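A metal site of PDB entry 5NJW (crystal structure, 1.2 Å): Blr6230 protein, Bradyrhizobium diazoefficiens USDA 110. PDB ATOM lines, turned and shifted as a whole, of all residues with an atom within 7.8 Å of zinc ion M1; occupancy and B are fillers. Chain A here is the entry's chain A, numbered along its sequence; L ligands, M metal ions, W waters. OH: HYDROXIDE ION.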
ATOM      1  N   PHE A  26     -23.169  21.668 -19.979  1.00  0.00           N
ATOM      2  CA  PHE A  26     -23.529  21.896 -18.575  1.00  0.00           C
ATOM      3  C   PHE A  26     -23.483  20.566 -17.800  1.00  0.00           C
ATOM      4  O   PHE A  26     -22.883  20.492 -16.687  1.00  0.00           O
ATOM      5  CB  PHE A  26     -24.906  22.561 -18.456  1.00  0.00           C
ATOM      6  CG  PHE A  26     -25.394  22.726 -17.044  1.00  0.00           C
ATOM      7  CD1 PHE A  26     -25.095  23.860 -16.305  1.00  0.00           C
ATOM      8  CD2 PHE A  26     -26.168  21.741 -16.451  1.00  0.00           C
ATOM      9  CE1 PHE A  26     -25.540  23.999 -14.993  1.00  0.00           C
ATOM     10  CE2 PHE A  26     -26.628  21.867 -15.143  1.00  0.00           C
ATOM     11  CZ  PHE A  26     -26.314  23.006 -14.420  1.00  0.00           C
ATOM     12  N   TRP A  34     -17.825  19.272 -10.961  1.00  0.00           N
ATOM     13  CA  TRP A  34     -18.699  19.646  -9.841  1.00  0.00           C
ATOM     14  C   TRP A  34     -18.963  18.554  -8.807  1.00  0.00           C
ATOM     15  O   TRP A  34     -19.505  18.835  -7.741  1.00  0.00           O
ATOM     16  CB  TRP A  34     -20.019  20.183 -10.399  1.00  0.00           C
ATOM     17  CG  TRP A  34     -19.882  21.510 -11.118  1.00  0.00           C
ATOM     18  CD1 TRP A  34     -18.722  22.195 -11.414  1.00  0.00           C
ATOM     19  CD2 TRP A  34     -20.936  22.287 -11.664  1.00  0.00           C
ATOM     20  NE1 TRP A  34     -19.021  23.352 -12.083  1.00  0.00           N
ATOM     21  CE2 TRP A  34     -20.369  23.449 -12.225  1.00  0.00           C
ATOM     22  CE3 TRP A  34     -22.311  22.139 -11.708  1.00  0.00           C
ATOM     23  CZ2 TRP A  34     -21.141  24.424 -12.868  1.00  0.00           C
ATOM     24  CZ3 TRP A  34     -23.070  23.114 -12.346  1.00  0.00           C
ATOM     25  CH2 TRP A  34     -22.479  24.240 -12.875  1.00  0.00           C
ATOM     26  N   THR A 100     -30.364  29.428  -2.268  1.00  0.00           N
ATOM     27  CA  THR A 100     -30.081  30.623  -3.054  1.00  0.00           C
ATOM     28  C   THR A 100     -30.978  30.621  -4.295  1.00  0.00           C
ATOM     29  O   THR A 100     -31.715  31.576  -4.550  1.00  0.00           O
ATOM     30  CB  THR A 100     -28.613  30.682  -3.516  1.00  0.00           C
ATOM     31  OG1 THR A 100     -28.237  29.431  -4.117  1.00  0.00           O
ATOM     32  CG2 THR A 100     -27.698  31.042  -2.372  1.00  0.00           C
ATOM     33  N   HIS A 101     -30.973  29.524  -5.073  1.00  0.00           N
ATOM     34  CA  HIS A 101     -31.864  29.439  -6.221  1.00  0.00           C
ATOM     35  C   HIS A 101     -32.090  27.976  -6.618  1.00  0.00           C
ATOM     36  O   HIS A 101     -31.283  27.074  -6.339  1.00  0.00           O
ATOM     37  CB  HIS A 101     -31.328  30.239  -7.417  1.00  0.00           C
ATOM     38  CG  HIS A 101     -30.160  29.609  -8.127  1.00  0.00           C
ATOM     39  ND1 HIS A 101     -28.847  29.894  -7.857  1.00  0.00           N
ATOM     40  CD2 HIS A 101     -30.133  28.738  -9.154  1.00  0.00           C
ATOM     41  CE1 HIS A 101     -28.057  29.221  -8.674  1.00  0.00           C
ATOM     42  NE2 HIS A 101     -28.818  28.484  -9.454  1.00  0.00           N
ATOM     43  N   ALA A 102     -33.226  27.741  -7.274  1.00  0.00           N
ATOM     44  CA  ALA A 102     -33.780  26.426  -7.437  1.00  0.00           C
ATOM     45  C   ALA A 102     -33.381  25.765  -8.741  1.00  0.00           C
ATOM     46  O   ALA A 102     -34.231  25.507  -9.599  1.00  0.00           O
ATOM     47  CB  ALA A 102     -35.299  26.533  -7.301  1.00  0.00           C
ATOM     48  N   HIS A 103     -32.094  25.481  -8.912  1.00  0.00           N
ATOM     49  CA  HIS A 103     -31.567  24.585  -9.965  1.00  0.00           C
ATOM     50  C   HIS A 103     -30.951  23.342  -9.366  1.00  0.00           C
ATOM     51  O   HIS A 103     -30.450  23.402  -8.211  1.00  0.00           O
ATOM     52  CB  HIS A 103     -30.512  25.298 -10.804  1.00  0.00           C
ATOM     53  CG  HIS A 103     -31.039  26.409 -11.640  1.00  0.00           C
ATOM     54  ND1 HIS A 103     -30.222  27.423 -12.102  1.00  0.00           N
ATOM     55  CD2 HIS A 103     -32.271  26.644 -12.152  1.00  0.00           C
ATOM     56  CE1 HIS A 103     -30.929  28.235 -12.863  1.00  0.00           C
ATOM     57  NE2 HIS A 103     -32.175  27.811 -12.888  1.00  0.00           N
ATOM     58  N   LEU A 104     -30.957  22.246 -10.116  1.00  0.00           N
ATOM     59  CA  LEU A 104     -30.564  20.937  -9.597  1.00  0.00           C
ATOM     60  C   LEU A 104     -29.173  20.871  -8.982  1.00  0.00           C
ATOM     61  O   LEU A 104     -28.944  20.027  -8.140  1.00  0.00           O
ATOM     62  CB  LEU A 104     -30.692  19.834 -10.648  1.00  0.00           C
ATOM     63  CG  LEU A 104     -29.599  19.676 -11.676  1.00  0.00           C
ATOM     64  CD1 LEU A 104     -29.741  18.293 -12.345  1.00  0.00           C
ATOM     65  CD2 LEU A 104     -29.639  20.823 -12.676  1.00  0.00           C
ATOM     66  N   ASP A 105     -28.241  21.693  -9.455  1.00  0.00           N
ATOM     67  CA  ASP A 105     -26.905  21.679  -8.905  1.00  0.00           C
ATOM     68  C   ASP A 105     -26.828  22.290  -7.486  1.00  0.00           C
ATOM     69  O   ASP A 105     -25.789  22.198  -6.840  1.00  0.00           O
ATOM     70  CB  ASP A 105     -25.887  22.306  -9.861  1.00  0.00           C
ATOM     71  CG  ASP A 105     -26.234  23.727 -10.325  1.00  0.00           C
ATOM     72  OD1 ASP A 105     -27.408  24.035 -10.616  1.00  0.00           O
ATOM     73  OD2 ASP A 105     -25.262  24.534 -10.442  1.00  0.00           O
ATOM     74  N   HIS A 106     -27.916  22.917  -7.013  1.00  0.00           N
ATOM     75  CA  HIS A 106     -28.004  23.474  -5.663  1.00  0.00           C
ATOM     76  C   HIS A 106     -29.096  22.819  -4.841  1.00  0.00           C
ATOM     77  O   HIS A 106     -29.080  22.934  -3.612  1.00  0.00           O
ATOM     78  CB  HIS A 106     -28.189  24.972  -5.719  1.00  0.00           C
ATOM     79  CG  HIS A 106     -27.189  25.595  -6.606  1.00  0.00           C
ATOM     80  ND1 HIS A 106     -25.849  25.631  -6.303  1.00  0.00           N
ATOM     81  CD2 HIS A 106     -27.302  26.110  -7.848  1.00  0.00           C
ATOM     82  CE1 HIS A 106     -25.182  26.130  -7.329  1.00  0.00           C
ATOM     83  NE2 HIS A 106     -26.050  26.459  -8.276  1.00  0.00           N
ATOM     84  N   TYR A 136     -36.743  22.451 -14.344  1.00  0.00           N
ATOM     85  CA  TYR A 136     -36.051  23.657 -14.808  1.00  0.00           C
ATOM     86  C   TYR A 136     -37.066  24.583 -15.518  1.00  0.00           C
ATOM     87  O   TYR A 136     -37.773  24.130 -16.420  1.00  0.00           O
ATOM     88  CB  TYR A 136     -34.914  23.299 -15.778  1.00  0.00           C
ATOM     89  CG  TYR A 136     -33.964  24.438 -15.972  1.00  0.00           C
ATOM     90  CD1 TYR A 136     -34.256  25.498 -16.858  1.00  0.00           C
ATOM     91  CD2 TYR A 136     -32.799  24.524 -15.234  1.00  0.00           C
ATOM     92  CE1 TYR A 136     -33.403  26.574 -16.999  1.00  0.00           C
ATOM     93  CE2 TYR A 136     -31.943  25.608 -15.364  1.00  0.00           C
ATOM     94  CZ  TYR A 136     -32.251  26.633 -16.233  1.00  0.00           C
ATOM     95  OH  TYR A 136     -31.370  27.695 -16.331  1.00  0.00           O
ATOM     96  N   HIS A 177     -31.144  34.903 -12.615  1.00  0.00           N
ATOM     97  CA  HIS A 177     -30.657  33.556 -12.838  1.00  0.00           C
ATOM     98  C   HIS A 177     -31.778  32.542 -12.575  1.00  0.00           C
ATOM     99  O   HIS A 177     -31.865  31.503 -13.240  1.00  0.00           O
ATOM    100  CB  HIS A 177     -29.410  33.327 -12.002  1.00  0.00           C
ATOM    101  CG  HIS A 177     -28.796  31.986 -12.200  1.00  0.00           C
ATOM    102  ND1 HIS A 177     -27.956  31.680 -13.240  1.00  0.00           N
ATOM    103  CD2 HIS A 177     -28.971  30.845 -11.515  1.00  0.00           C
ATOM    104  CE1 HIS A 177     -27.576  30.425 -13.145  1.00  0.00           C
ATOM    105  NE2 HIS A 177     -28.206  29.874 -12.124  1.00  0.00           N
ATOM    106  N   SER A 178     -32.658  32.842 -11.613  1.00  0.00           N
ATOM    107  CA  SER A 178     -33.925  32.133 -11.441  1.00  0.00           C
ATOM    108  C   SER A 178     -34.932  33.186 -10.979  1.00  0.00           C
ATOM    109  O   SER A 178     -34.532  34.257 -10.498  1.00  0.00           O
ATOM    110  CB  SER A 178     -33.847  31.005 -10.396  1.00  0.00           C
ATOM    111  OG  SER A 178     -33.823  31.540  -9.068  1.00  0.00           O
ATOM    112  N   CYS A 181     -34.521  33.815  -7.152  1.00  0.00           N
ATOM    113  CA  CYS A 181     -33.116  33.816  -6.685  1.00  0.00           C
ATOM    114  C   CYS A 181     -32.998  34.795  -5.503  1.00  0.00           C
ATOM    115  O   CYS A 181     -33.377  35.956  -5.636  1.00  0.00           O
ATOM    116  CB  CYS A 181     -32.252  34.270  -7.881  1.00  0.00           C
ATOM    117  SG  CYS A 181     -30.536  33.781  -8.032  1.00  0.00           S
ATOM    118  N   CYS A 201     -26.770  34.882  -4.883  1.00  0.00           N
ATOM    119  CA  CYS A 201     -27.502  33.739  -5.398  1.00  0.00           C
ATOM    120  C   CYS A 201     -27.058  33.203  -6.724  1.00  0.00           C
ATOM    121  O   CYS A 201     -27.449  32.100  -7.050  1.00  0.00           O
ATOM    122  CB  CYS A 201     -28.989  34.038  -5.441  1.00  0.00           C
ATOM    123  SG  CYS A 201     -29.515  35.131  -6.747  1.00  0.00           S
ATOM    124  N   SER A 202     -26.310  34.002  -7.478  1.00  0.00           N
ATOM    125  CA  SER A 202     -25.871  33.783  -8.885  1.00  0.00           C
ATOM    126  C   SER A 202     -26.481  34.826  -9.792  1.00  0.00           C
ATOM    127  O   SER A 202     -27.702  35.098  -9.703  1.00  0.00           O
ATOM    128  CB  SER A 202     -26.248  32.451  -9.547  1.00  0.00           C
ATOM    129  OG  SER A 202     -25.866  32.505 -10.924  1.00  0.00           O
ATOM    130  N   THR A 204     -25.311  34.656 -13.374  1.00  0.00           N
ATOM    131  CA  THR A 204     -24.876  34.198 -14.686  1.00  0.00           C
ATOM    132  C   THR A 204     -26.102  33.949 -15.588  1.00  0.00           C
ATOM    133  O   THR A 204     -27.191  33.654 -15.123  1.00  0.00           O
ATOM    134  CB  THR A 204     -24.072  32.889 -14.559  1.00  0.00           C
ATOM    135  OG1 THR A 204     -24.942  31.887 -14.054  1.00  0.00           O
ATOM    136  CG2 THR A 204     -22.853  33.075 -13.667  1.00  0.00           C
ATOM    137  N   VAL A 205     -25.901  34.067 -16.896  1.00  0.00           N
ATOM    138  CA  VAL A 205     -26.921  33.717 -17.877  1.00  0.00           C
ATOM    139  C   VAL A 205     -27.092  32.201 -17.984  1.00  0.00           C
ATOM    140  O   VAL A 205     -28.216  31.699 -17.982  1.00  0.00           O
ATOM    141  CB  VAL A 205     -26.620  34.351 -19.259  1.00  0.00           C
ATOM    142  CG1 VAL A 205     -27.601  33.863 -20.304  1.00  0.00           C
ATOM    143  CG2 VAL A 205     -26.698  35.854 -19.136  1.00  0.00           C
ATOM    144  N   ALA A 206     -25.966  31.490 -18.066  1.00  0.00           N
ATOM    145  CA  ALA A 206     -25.928  30.035 -18.035  1.00  0.00           C
ATOM    146  C   ALA A 206     -26.889  29.454 -19.089  1.00  0.00           C
ATOM    147  O   ALA A 206     -26.719  29.803 -20.281  1.00  0.00           O
ATOM    148  CB  ALA A 206     -26.160  29.554 -16.613  1.00  0.00           C
ATOM    149  N   LEU A 207     -27.840  28.609 -18.707  1.00  0.00           N
ATOM    150  CA  LEU A 207     -28.746  27.977 -19.653  1.00  0.00           C
ATOM    151  C   LEU A 207     -30.003  28.787 -19.934  1.00  0.00           C
ATOM    152  O   LEU A 207     -30.842  28.353 -20.705  1.00  0.00           O
ATOM    153  CB  LEU A 207     -29.155  26.598 -19.161  1.00  0.00           C
ATOM    154  CG  LEU A 207     -28.027  25.589 -18.950  1.00  0.00           C
ATOM    155  CD1 LEU A 207     -28.649  24.295 -18.403  1.00  0.00           C
ATOM    156  CD2 LEU A 207     -27.225  25.343 -20.221  1.00  0.00           C
ATOM    157  N   ASN A 208     -30.166  29.961 -19.326  1.00  0.00           N
ATOM    158  CA  ASN A 208     -31.388  30.714 -19.506  1.00  0.00           C
ATOM    159  C   ASN A 208     -31.522  31.325 -20.920  1.00  0.00           C
ATOM    160  O   ASN A 208     -30.532  31.765 -21.503  1.00  0.00           O
ATOM    161  CB  ASN A 208     -31.518  31.805 -18.454  1.00  0.00           C
ATOM    162  CG  ASN A 208     -31.765  31.245 -17.067  1.00  0.00           C
ATOM    163  OD1 ASN A 208     -32.369  30.175 -16.919  1.00  0.00           O
ATOM    164  ND2 ASN A 208     -31.274  31.948 -16.054  1.00  0.00           N
ATOM    165  N   PRO A 241     -22.890  30.412  -4.871  1.00  0.00           N
ATOM    166  CA  PRO A 241     -23.233  28.979  -4.950  1.00  0.00           C
ATOM    167  C   PRO A 241     -22.246  28.152  -5.750  1.00  0.00           C
ATOM    168  O   PRO A 241     -22.405  26.935  -5.804  1.00  0.00           O
ATOM    169  CB  PRO A 241     -24.605  28.971  -5.630  1.00  0.00           C
ATOM    170  CG  PRO A 241     -24.837  30.284  -6.132  1.00  0.00           C
ATOM    171  CD  PRO A 241     -23.786  31.235  -5.692  1.00  0.00           C
ATOM    172  N   HIS A 242     -21.266  28.797  -6.379  1.00  0.00           N
ATOM    173  CA  HIS A 242     -20.135  28.129  -6.994  1.00  0.00           C
ATOM    174  C   HIS A 242     -18.885  28.848  -6.491  1.00  0.00           C
ATOM    175  O   HIS A 242     -18.894  30.071  -6.372  1.00  0.00           O
ATOM    176  CB  HIS A 242     -20.230  28.203  -8.528  1.00  0.00           C
ATOM    177  CG  HIS A 242     -21.387  27.440  -9.102  1.00  0.00           C
ATOM    178  ND1 HIS A 242     -21.367  26.073  -9.274  1.00  0.00           N
ATOM    179  CD2 HIS A 242     -22.611  27.848  -9.491  1.00  0.00           C
ATOM    180  CE1 HIS A 242     -22.527  25.667  -9.749  1.00  0.00           C
ATOM    181  NE2 HIS A 242     -23.299  26.726  -9.894  1.00  0.00           N
HETATM  182  O    OH L   1     -27.005  26.639 -11.479  1.00  0.00           O
HETATM  183 ZN    ZN M   1     -28.310  27.950 -11.375  1.00  0.00          ZN
HETATM  184 ZN    ZN M   2     -25.397  26.624 -10.241  1.00  0.00          ZN
HETATM  185  O   HOH W   1     -26.621  27.221 -14.141  1.00  0.00           O
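A ring nitrogen (ND1) of His 101 sits at hydrogen-bond distance from the backbone carbonyl oxygen of Cys 201, 2.7 Å away. A ring nitrogen (ND1) of His 177 sits at hydrogen-bond distance from the side-chain hydroxyl (OG) of Ser 202. The backbone carbonyl oxygen of Thr 204 lies within hydrogen-bond range of a ring nitrogen (ND1) of His 177 (2.8 Å). The backbone carbonyl oxygen (O) of His 177 lies within hydrogen-bond range of the side-chain amide nitrogen (ND2) of Asn 208, at 2.9 Å. The side-chain sulfur (SG) of Cys 201 is disulfide-bonded to the side-chain sulfur (SG) of Cys 181, at 2.1 Å.
Zinc ion M1 is bound by an oxygen (O) of the ligand. Zinc ion M1 is bound by a ring nitrogen (NE2) of His 101 (2.1 Å). NE2 of His 177 binds zinc ion M1, 2.1 Å away. ND1 of His 103 binds zinc ion M1 (2.1 Å).
Three residues have an atom within 4 Å of zinc ion M1: His 101, His 103 and His 177. Along chain A the residues within 4 Å of zinc ion M1 span positions 101 to 177. The nearest printed residue that does not touch zinc ion M1 is Asp 105 (4.1 Å).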
